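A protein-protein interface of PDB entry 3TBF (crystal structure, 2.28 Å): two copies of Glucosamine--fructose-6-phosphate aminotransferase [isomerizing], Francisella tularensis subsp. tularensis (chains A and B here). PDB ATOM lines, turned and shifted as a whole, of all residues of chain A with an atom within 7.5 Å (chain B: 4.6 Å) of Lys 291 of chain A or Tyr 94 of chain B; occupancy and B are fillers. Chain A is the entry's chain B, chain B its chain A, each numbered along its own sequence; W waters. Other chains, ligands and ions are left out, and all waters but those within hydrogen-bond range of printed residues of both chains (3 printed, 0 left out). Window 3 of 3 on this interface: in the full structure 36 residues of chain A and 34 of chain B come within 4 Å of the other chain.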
ATOM      1  N   TYR A  74     -21.019   8.041 -29.422  1.00  0.00           N
ATOM      2  CA  TYR A  74     -19.599   7.918 -29.151  1.00  0.00           C
ATOM      3  C   TYR A  74     -18.798   8.239 -30.398  1.00  0.00           C
ATOM      4  O   TYR A  74     -17.815   8.977 -30.326  1.00  0.00           O
ATOM      5  CB  TYR A  74     -19.257   6.522 -28.660  1.00  0.00           C
ATOM      6  CG  TYR A  74     -19.664   6.255 -27.233  1.00  0.00           C
ATOM      7  CD1 TYR A  74     -20.963   5.921 -26.935  1.00  0.00           C
ATOM      8  CD2 TYR A  74     -18.738   6.351 -26.166  1.00  0.00           C
ATOM      9  CE1 TYR A  74     -21.386   5.704 -25.639  1.00  0.00           C
ATOM     10  CE2 TYR A  74     -19.146   6.092 -24.849  1.00  0.00           C
ATOM     11  CZ  TYR A  74     -20.478   5.778 -24.603  1.00  0.00           C
ATOM     12  OH  TYR A  74     -20.914   5.520 -23.337  1.00  0.00           O
ATOM     13  N   ARG A 235     -18.564  -1.084 -21.433  1.00  0.00           N
ATOM     14  CA  ARG A 235     -18.102   0.248 -21.151  1.00  0.00           C
ATOM     15  C   ARG A 235     -17.975   0.958 -22.473  1.00  0.00           C
ATOM     16  O   ARG A 235     -17.672   0.354 -23.470  1.00  0.00           O
ATOM     17  CB  ARG A 235     -16.704   0.224 -20.559  1.00  0.00           C
ATOM     18  CG  ARG A 235     -16.627   0.204 -19.064  1.00  0.00           C
ATOM     19  CD  ARG A 235     -15.172   0.293 -18.618  1.00  0.00           C
ATOM     20  NE  ARG A 235     -15.074   0.455 -17.191  1.00  0.00           N
ATOM     21  CZ  ARG A 235     -15.091   1.627 -16.557  1.00  0.00           C
ATOM     22  NH1 ARG A 235     -15.188   2.793 -17.216  1.00  0.00           N
ATOM     23  NH2 ARG A 235     -15.011   1.623 -15.244  1.00  0.00           N
ATOM     24  N   GLY A 236     -18.112   2.278 -22.431  1.00  0.00           N
ATOM     25  CA  GLY A 236     -17.948   3.126 -23.605  1.00  0.00           C
ATOM     26  C   GLY A 236     -18.932   2.715 -24.661  1.00  0.00           C
ATOM     27  O   GLY A 236     -20.094   2.417 -24.366  1.00  0.00           O
ATOM     28  N   SER A 262     -20.005  -0.878 -16.893  1.00  0.00           N
ATOM     29  CA  SER A 262     -19.124  -1.590 -15.966  1.00  0.00           C
ATOM     30  C   SER A 262     -18.563  -0.729 -14.852  1.00  0.00           C
ATOM     31  O   SER A 262     -18.365  -1.244 -13.761  1.00  0.00           O
ATOM     32  CB  SER A 262     -17.971  -2.263 -16.680  1.00  0.00           C
ATOM     33  OG  SER A 262     -18.464  -2.905 -17.829  1.00  0.00           O
ATOM     34  N   GLY A 263     -18.353   0.565 -15.110  1.00  0.00           N
ATOM     35  CA  GLY A 263     -17.938   1.522 -14.084  1.00  0.00           C
ATOM     36  C   GLY A 263     -18.918   1.797 -12.944  1.00  0.00           C
ATOM     37  O   GLY A 263     -18.562   2.454 -11.981  1.00  0.00           O
ATOM     38  N   LYS A 266     -20.519  -0.238  -8.702  1.00  0.00           N
ATOM     39  CA  LYS A 266     -20.185   0.240  -7.349  1.00  0.00           C
ATOM     40  C   LYS A 266     -21.368   0.932  -6.695  1.00  0.00           C
ATOM     41  O   LYS A 266     -21.201   1.958  -6.050  1.00  0.00           O
ATOM     42  CB  LYS A 266     -18.988   1.234  -7.360  1.00  0.00           C
ATOM     43  CG  LYS A 266     -17.939   1.095  -8.477  1.00  0.00           C
ATOM     44  CD  LYS A 266     -17.300  -0.295  -8.544  1.00  0.00           C
ATOM     45  CE  LYS A 266     -16.814  -0.597  -9.970  1.00  0.00           C
ATOM     46  NZ  LYS A 266     -17.932  -0.697 -10.959  1.00  0.00           N
ATOM     47  N   GLU A 287      -8.569   0.952 -24.873  1.00  0.00           N
ATOM     48  CA  GLU A 287      -7.776   1.477 -23.728  1.00  0.00           C
ATOM     49  C   GLU A 287      -8.362   1.150 -22.370  1.00  0.00           C
ATOM     50  O   GLU A 287      -7.695   1.250 -21.341  1.00  0.00           O
ATOM     51  CB  GLU A 287      -7.675   2.998 -23.792  1.00  0.00           C
ATOM     52  CG  GLU A 287      -7.382   3.572 -25.187  1.00  0.00           C
ATOM     53  CD  GLU A 287      -7.838   5.044 -25.338  1.00  0.00           C
ATOM     54  OE1 GLU A 287      -8.986   5.374 -24.893  1.00  0.00           O
ATOM     55  OE2 GLU A 287      -7.043   5.854 -25.917  1.00  0.00           O
ATOM     56  N   LEU A 288      -9.635   0.800 -22.372  1.00  0.00           N
ATOM     57  CA  LEU A 288     -10.375   0.574 -21.138  1.00  0.00           C
ATOM     58  C   LEU A 288     -10.277  -0.852 -20.620  1.00  0.00           C
ATOM     59  O   LEU A 288     -10.941  -1.229 -19.659  1.00  0.00           O
ATOM     60  CB  LEU A 288     -11.826   0.957 -21.346  1.00  0.00           C
ATOM     61  CG  LEU A 288     -12.052   2.415 -21.747  1.00  0.00           C
ATOM     62  CD1 LEU A 288     -13.554   2.725 -21.690  1.00  0.00           C
ATOM     63  CD2 LEU A 288     -11.203   3.366 -20.829  1.00  0.00           C
ATOM     64  N   LEU A 289      -9.401  -1.629 -21.233  1.00  0.00           N
ATOM     65  CA  LEU A 289      -9.286  -3.010 -20.885  1.00  0.00           C
ATOM     66  C   LEU A 289      -8.890  -3.153 -19.434  1.00  0.00           C
ATOM     67  O   LEU A 289      -9.449  -3.987 -18.727  1.00  0.00           O
ATOM     68  CB  LEU A 289      -8.292  -3.713 -21.814  1.00  0.00           C
ATOM     69  CG  LEU A 289      -8.070  -5.157 -21.391  1.00  0.00           C
ATOM     70  CD1 LEU A 289      -9.249  -6.027 -21.837  1.00  0.00           C
ATOM     71  CD2 LEU A 289      -6.700  -5.666 -21.893  1.00  0.00           C
ATOM     72  N   ASP A 290      -7.961  -2.323 -18.968  1.00  0.00           N
ATOM     73  CA  ASP A 290      -7.500  -2.459 -17.601  1.00  0.00           C
ATOM     74  C   ASP A 290      -8.662  -2.218 -16.652  1.00  0.00           C
ATOM     75  O   ASP A 290      -8.948  -3.054 -15.793  1.00  0.00           O
ATOM     76  CB  ASP A 290      -6.292  -1.545 -17.305  1.00  0.00           C
ATOM     77  CG  ASP A 290      -4.955  -2.068 -17.943  1.00  0.00           C
ATOM     78  OD1 ASP A 290      -4.743  -3.313 -18.060  1.00  0.00           O
ATOM     79  OD2 ASP A 290      -4.095  -1.224 -18.312  1.00  0.00           O
ATOM     80  N   LYS A 291      -9.382  -1.119 -16.800  1.00  0.00           N
ATOM     81  CA  LYS A 291     -10.516  -0.962 -15.892  1.00  0.00           C
ATOM     82  C   LYS A 291     -11.655  -2.002 -16.052  1.00  0.00           C
ATOM     83  O   LYS A 291     -12.178  -2.475 -15.061  1.00  0.00           O
ATOM     84  CB  LYS A 291     -11.006   0.467 -15.845  1.00  0.00           C
ATOM     85  CG  LYS A 291     -11.409   1.040 -17.127  1.00  0.00           C
ATOM     86  CD  LYS A 291     -11.386   2.545 -17.033  1.00  0.00           C
ATOM     87  CE  LYS A 291     -10.082   3.081 -17.556  1.00  0.00           C
ATOM     88  NZ  LYS A 291      -9.038   3.025 -16.481  1.00  0.00           N
ATOM     89  N   THR A 292     -11.977  -2.417 -17.273  1.00  0.00           N
ATOM     90  CA  THR A 292     -12.971  -3.485 -17.470  1.00  0.00           C
ATOM     91  C   THR A 292     -12.533  -4.741 -16.730  1.00  0.00           C
ATOM     92  O   THR A 292     -13.328  -5.385 -16.088  1.00  0.00           O
ATOM     93  CB  THR A 292     -13.152  -3.801 -18.949  1.00  0.00           C
ATOM     94  OG1 THR A 292     -13.793  -2.695 -19.589  1.00  0.00           O
ATOM     95  CG2 THR A 292     -13.971  -5.107 -19.208  1.00  0.00           C
ATOM     96  N   LEU A 293     -11.251  -5.083 -16.823  1.00  0.00           N
ATOM     97  CA  LEU A 293     -10.744  -6.263 -16.129  1.00  0.00           C
ATOM     98  C   LEU A 293     -10.909  -6.126 -14.611  1.00  0.00           C
ATOM     99  O   LEU A 293     -11.292  -7.092 -13.951  1.00  0.00           O
ATOM    100  CB  LEU A 293      -9.274  -6.537 -16.495  1.00  0.00           C
ATOM    101  CG  LEU A 293      -9.010  -7.070 -17.903  1.00  0.00           C
ATOM    102  CD1 LEU A 293      -7.539  -7.446 -18.070  1.00  0.00           C
ATOM    103  CD2 LEU A 293      -9.863  -8.255 -18.238  1.00  0.00           C
ATOM    104  N   SER A 294     -10.668  -4.932 -14.063  1.00  0.00           N
ATOM    105  CA  SER A 294     -10.899  -4.717 -12.617  1.00  0.00           C
ATOM    106  C   SER A 294     -12.355  -4.888 -12.331  1.00  0.00           C
ATOM    107  O   SER A 294     -12.707  -5.624 -11.418  1.00  0.00           O
ATOM    108  CB  SER A 294     -10.459  -3.326 -12.103  1.00  0.00           C
ATOM    109  OG  SER A 294      -9.285  -2.872 -12.762  1.00  0.00           O
ATOM    110  N   ASN A 295     -13.210  -4.221 -13.086  1.00  0.00           N
ATOM    111  CA  ASN A 295     -14.666  -4.386 -12.882  1.00  0.00           C
ATOM    112  C   ASN A 295     -15.101  -5.857 -12.846  1.00  0.00           C
ATOM    113  O   ASN A 295     -15.838  -6.274 -11.981  1.00  0.00           O
ATOM    114  CB  ASN A 295     -15.468  -3.658 -13.960  1.00  0.00           C
ATOM    115  CG  ASN A 295     -15.297  -2.160 -13.914  1.00  0.00           C
ATOM    116  OD1 ASN A 295     -15.306  -1.484 -14.952  1.00  0.00           O
ATOM    117  ND2 ASN A 295     -15.135  -1.624 -12.706  1.00  0.00           N
ATOM    118  N   LEU A 296     -14.632  -6.635 -13.803  1.00  0.00           N
ATOM    119  CA  LEU A 296     -14.938  -8.052 -13.866  1.00  0.00           C
ATOM    120  C   LEU A 296     -14.428  -8.836 -12.672  1.00  0.00           C
ATOM    121  O   LEU A 296     -15.040  -9.811 -12.266  1.00  0.00           O
ATOM    122  CB  LEU A 296     -14.308  -8.646 -15.110  1.00  0.00           C
ATOM    123  CG  LEU A 296     -14.907  -8.166 -16.418  1.00  0.00           C
ATOM    124  CD1 LEU A 296     -14.104  -8.774 -17.556  1.00  0.00           C
ATOM    125  CD2 LEU A 296     -16.374  -8.554 -16.466  1.00  0.00           C
ATOM    126  N   GLN A 297     -13.279  -8.426 -12.148  1.00  0.00           N
ATOM    127  CA  GLN A 297     -12.706  -9.028 -10.956  1.00  0.00           C
ATOM    128  C   GLN A 297     -13.661  -8.961  -9.778  1.00  0.00           C
ATOM    129  O   GLN A 297     -13.938  -9.962  -9.154  1.00  0.00           O
ATOM    130  CB  GLN A 297     -11.392  -8.327 -10.587  1.00  0.00           C
ATOM    131  CG  GLN A 297     -10.667  -8.935  -9.371  1.00  0.00           C
ATOM    132  CD  GLN A 297     -10.528 -10.460  -9.464  1.00  0.00           C
ATOM    133  OE1 GLN A 297     -10.082 -11.027 -10.494  1.00  0.00           O
ATOM    134  NE2 GLN A 297     -10.911 -11.133  -8.378  1.00  0.00           N
ATOM    135  N   GLU A 298     -14.160  -7.774  -9.502  1.00  0.00           N
ATOM    136  CA  GLU A 298     -15.092  -7.571  -8.415  1.00  0.00           C
ATOM    137  C   GLU A 298     -16.365  -8.390  -8.604  1.00  0.00           C
ATOM    138  O   GLU A 298     -16.899  -8.940  -7.656  1.00  0.00           O
ATOM    139  CB  GLU A 298     -15.477  -6.092  -8.293  1.00  0.00           C
ATOM    140  CG  GLU A 298     -14.291  -5.114  -8.257  1.00  0.00           C
ATOM    141  CD  GLU A 298     -14.737  -3.646  -8.253  1.00  0.00           C
ATOM    142  OE1 GLU A 298     -14.974  -3.091  -7.132  1.00  0.00           O
ATOM    143  OE2 GLU A 298     -14.837  -3.049  -9.369  1.00  0.00           O
ATOM    144  N   SER B  90     -18.534   7.901 -14.768  1.00  0.00           N
ATOM    145  CA  SER B  90     -17.567   6.904 -15.160  1.00  0.00           C
ATOM    146  C   SER B  90     -17.500   6.710 -16.646  1.00  0.00           C
ATOM    147  O   SER B  90     -16.536   6.105 -17.129  1.00  0.00           O
ATOM    148  CB  SER B  90     -17.884   5.580 -14.522  1.00  0.00           C
ATOM    149  OG  SER B  90     -19.055   5.019 -15.083  1.00  0.00           O
ATOM    150  N   GLU B  91     -18.470   7.249 -17.388  1.00  0.00           N
ATOM    151  CA  GLU B  91     -18.405   7.205 -18.858  1.00  0.00           C
ATOM    152  C   GLU B  91     -17.814   8.468 -19.447  1.00  0.00           C
ATOM    153  O   GLU B  91     -16.932   8.357 -20.331  1.00  0.00           O
ATOM    154  CB  GLU B  91     -19.769   6.945 -19.450  1.00  0.00           C
ATOM    155  CG  GLU B  91     -20.204   5.522 -19.180  1.00  0.00           C
ATOM    156  CD  GLU B  91     -19.475   4.515 -20.101  1.00  0.00           C
ATOM    157  OE1 GLU B  91     -19.320   4.874 -21.281  1.00  0.00           O
ATOM    158  OE2 GLU B  91     -19.055   3.408 -19.675  1.00  0.00           O
ATOM    159  N   ILE B  92     -18.247   9.655 -18.994  1.00  0.00           N
ATOM    160  CA  ILE B  92     -17.748  10.874 -19.609  1.00  0.00           C
ATOM    161  C   ILE B  92     -16.277  11.043 -19.321  1.00  0.00           C
ATOM    162  O   ILE B  92     -15.531  11.636 -20.113  1.00  0.00           O
ATOM    163  CB  ILE B  92     -18.523  12.147 -19.210  1.00  0.00           C
ATOM    164  CG1 ILE B  92     -18.182  13.312 -20.143  1.00  0.00           C
ATOM    165  CG2 ILE B  92     -18.302  12.559 -17.764  1.00  0.00           C
ATOM    166  CD1 ILE B  92     -18.959  14.592 -19.680  1.00  0.00           C
ATOM    167  N   ARG B  93     -15.839  10.502 -18.197  1.00  0.00           N
ATOM    168  CA  ARG B  93     -14.427  10.645 -17.774  1.00  0.00           C
ATOM    169  C   ARG B  93     -13.430  10.134 -18.814  1.00  0.00           C
ATOM    170  O   ARG B  93     -12.403  10.747 -19.075  1.00  0.00           O
ATOM    171  CB  ARG B  93     -14.220   9.861 -16.493  1.00  0.00           C
ATOM    172  CG  ARG B  93     -12.870   9.934 -15.986  1.00  0.00           C
ATOM    173  CD  ARG B  93     -12.699   9.095 -14.749  1.00  0.00           C
ATOM    174  NE  ARG B  93     -11.309   9.157 -14.296  1.00  0.00           N
ATOM    175  CZ  ARG B  93     -10.870   8.489 -13.248  1.00  0.00           C
ATOM    176  NH1 ARG B  93     -11.724   7.760 -12.559  1.00  0.00           N
ATOM    177  NH2 ARG B  93      -9.604   8.543 -12.890  1.00  0.00           N
ATOM    178  N   TYR B  94     -13.762   8.989 -19.395  1.00  0.00           N
ATOM    179  CA  TYR B  94     -12.900   8.320 -20.359  1.00  0.00           C
ATOM    180  C   TYR B  94     -13.343   8.485 -21.789  1.00  0.00           C
ATOM    181  O   TYR B  94     -12.714   7.960 -22.654  1.00  0.00           O
ATOM    182  CB  TYR B  94     -12.848   6.847 -20.029  1.00  0.00           C
ATOM    183  CG  TYR B  94     -12.287   6.560 -18.658  1.00  0.00           C
ATOM    184  CD1 TYR B  94     -13.096   6.008 -17.661  1.00  0.00           C
ATOM    185  CD2 TYR B  94     -10.960   6.846 -18.348  1.00  0.00           C
ATOM    186  CE1 TYR B  94     -12.622   5.779 -16.392  1.00  0.00           C
ATOM    187  CE2 TYR B  94     -10.449   6.600 -17.062  1.00  0.00           C
ATOM    188  CZ  TYR B  94     -11.298   6.073 -16.096  1.00  0.00           C
ATOM    189  OH  TYR B  94     -10.813   5.822 -14.838  1.00  0.00           O
ATOM    190  N   ARG B  95     -14.386   9.249 -22.061  1.00  0.00           N
ATOM    191  CA  ARG B  95     -14.919   9.353 -23.395  1.00  0.00           C
ATOM    192  C   ARG B  95     -14.372  10.586 -24.070  1.00  0.00           C
ATOM    193  O   ARG B  95     -14.101  11.593 -23.444  1.00  0.00           O
ATOM    194  CB  ARG B  95     -16.435   9.434 -23.332  1.00  0.00           C
ATOM    195  CG  ARG B  95     -17.143   9.594 -24.622  1.00  0.00           C
ATOM    196  CD  ARG B  95     -18.620   9.403 -24.438  1.00  0.00           C
ATOM    197  NE  ARG B  95     -19.351  10.582 -23.979  1.00  0.00           N
ATOM    198  CZ  ARG B  95     -19.522  11.687 -24.713  1.00  0.00           C
ATOM    199  NH1 ARG B  95     -18.992  11.795 -25.934  1.00  0.00           N
ATOM    200  NH2 ARG B  95     -20.196  12.712 -24.222  1.00  0.00           N
ATOM    201  N   ASP B  96     -14.245  10.496 -25.382  1.00  0.00           N
ATOM    202  CA  ASP B  96     -13.690  11.562 -26.165  1.00  0.00           C
ATOM    203  C   ASP B  96     -14.837  12.507 -26.584  1.00  0.00           C
ATOM    204  O   ASP B  96     -15.376  12.382 -27.706  1.00  0.00           O
ATOM    205  CB  ASP B  96     -12.998  10.912 -27.359  1.00  0.00           C
ATOM    206  CG  ASP B  96     -11.914  11.771 -27.939  1.00  0.00           C
ATOM    207  OD1 ASP B  96     -12.134  13.006 -27.896  1.00  0.00           O
ATOM    208  OD2 ASP B  96     -10.868  11.217 -28.439  1.00  0.00           O
ATOM    209  N   ASP B 116     -14.879   9.395  -9.854  1.00  0.00           N
ATOM    210  CA  ASP B 116     -15.164   9.670 -11.254  1.00  0.00           C
ATOM    211  C   ASP B 116     -15.718  11.086 -11.514  1.00  0.00           C
ATOM    212  O   ASP B 116     -15.326  11.760 -12.475  1.00  0.00           O
ATOM    213  CB  ASP B 116     -16.134   8.619 -11.786  1.00  0.00           C
ATOM    214  CG  ASP B 116     -15.473   7.223 -11.964  1.00  0.00           C
ATOM    215  OD1 ASP B 116     -14.255   7.135 -12.279  1.00  0.00           O
ATOM    216  OD2 ASP B 116     -16.203   6.212 -11.812  1.00  0.00           O
HETATM  217  O   HOH W   1     -17.146   9.913 -27.760  1.00  0.00           O
HETATM  218  O   HOH W   2     -16.162   4.058 -19.270  1.00  0.00           O
HETATM  219  O   HOH W   3     -18.684   2.645 -16.943  1.00  0.00           O
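Water W2 lies within hydrogen-bond range of the guanidinium group of Arg 235 of chain A, the backbone carbonyl oxygen of Ser 90 of chain B and the side-chain carboxylate of Glu 91 of chain B.
Water W3 lies within hydrogen-bond range of the backbone NH of Gly 263 of chain A (2.8 Å), the side-chain carboxylate of Glu 91 of chain B (2.9 Å) and the side-chain hydroxyl of Ser 90 of chain B (3.0 Å).
Water W1 lies within hydrogen-bond range of the backbone carbonyl oxygen of Tyr 74 of chain A (2.8 Å), the backbone carbonyl oxygen of Asp 96 of chain B (3.0 Å) and the guanidinium group of Arg 95 of chain B (3.2 Å).
OH of Tyr 74 of chain A lies within hydrogen-bond range of O of Gly 236 of chain A (3.4 Å).
O of Leu 288 of chain A sits at hydrogen-bond distance from OG1 of Thr 292 of chain A, at 3.2 Å.
The backbone carbonyl oxygen of Lys 291 of chain A sits close to the side-chain amide oxygen of Asn 295 of chain A (3.3 Å).
O of Gly 263 of chain A sits close to NZ of Lys 266 of chain A, at 3.4 Å.
NH1 of Arg 93 of chain B lies close to OH of Tyr 94 of chain B, at 3.1 Å.
NE of Arg 235 of chain A sits at hydrogen-bond distance from OD1 of Asn 295 of chain A (3.0 Å).
No position is printed for both chains.
Of the 9 pairs that touch across the chains among the printed residues, none has its exchanged pair printed and touching as well.
Tyr 74 of chain A touches Arg 95 of chain B.
Arg 235 of chain A touches Ser 90 of chain B (NH1 to O, 3.6 Å).
Arg 235 of chain A touches Glu 91 of chain B (CA to OE2, 3.6 Å).
Tyr 94 of chain B touches Arg 235 of chain A (CD1 to NH1, 3.9 Å).
Ser 90 of chain B touches Gly 263 of chain A.
CD2 of Leu 288 of chain A touches CB of Tyr 94 of chain B (3.9 Å).
CD of Lys 291 of chain A touches CE1 of Tyr 94 of chain B, at 3.5 Å.
Of the printed residues of chain B, Tyr 74 of chain A touches Glu 91 (2.7 Å) and Arg 95 (3.4 Å).
Of the printed residues of chain B, Arg 235 of chain A touches Ser 90 (3.6 Å), Glu 91 (3.6 Å) and Tyr 94 (3.9 Å).
Printed residues of chain B within 4 Å of Gly 236 of chain A: Glu 91 (3.1 Å).
Printed residues of chain B within 4 Å of Leu 288 of chain A: Tyr 94.
Of chain B, only Tyr 94 comes within 4 Å of Lys 291 of chain A.
Printed residues of chain A within 4 Å of Arg 95 of chain B: Tyr 74.
The nearest residue of chain A that does not touch Tyr 94 of chain B is Glu 287 of chain A (5.1 Å).
The nearest printed residue of chain B that does not touch Tyr 74 of chain A is Asp 96 of chain B (4.9 Å).
Of the 18 printed residues of chain A, 6 touch a printed residue of chain B.
Of the 8 printed residues of chain B, 4 touch a printed residue of chain A.
Printed residues of chain B that touch a printed residue of chain A: Ser 90, Glu 91, Tyr 94 and Arg 95.
Hydrophobic or aromatic side chains of chain B within 4 Å of the printed part of chain A: Tyr 94.
Among the printed residues, 9 pairs touch across the chains.
Among the printed residues, no Asp or Glu carboxylate lies within 4 Å of a Lys or Arg side-chain nitrogen of the other chain.
The side-chain hydroxyl (OH) of Tyr 74 of chain A sits at hydrogen-bond distance from the side-chain carboxylate (OE1) of Glu 91 of chain B, at 2.7 Å.
OE1 of Glu 91 of chain B lies within hydrogen-bond range of N of Gly 236 of chain A.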
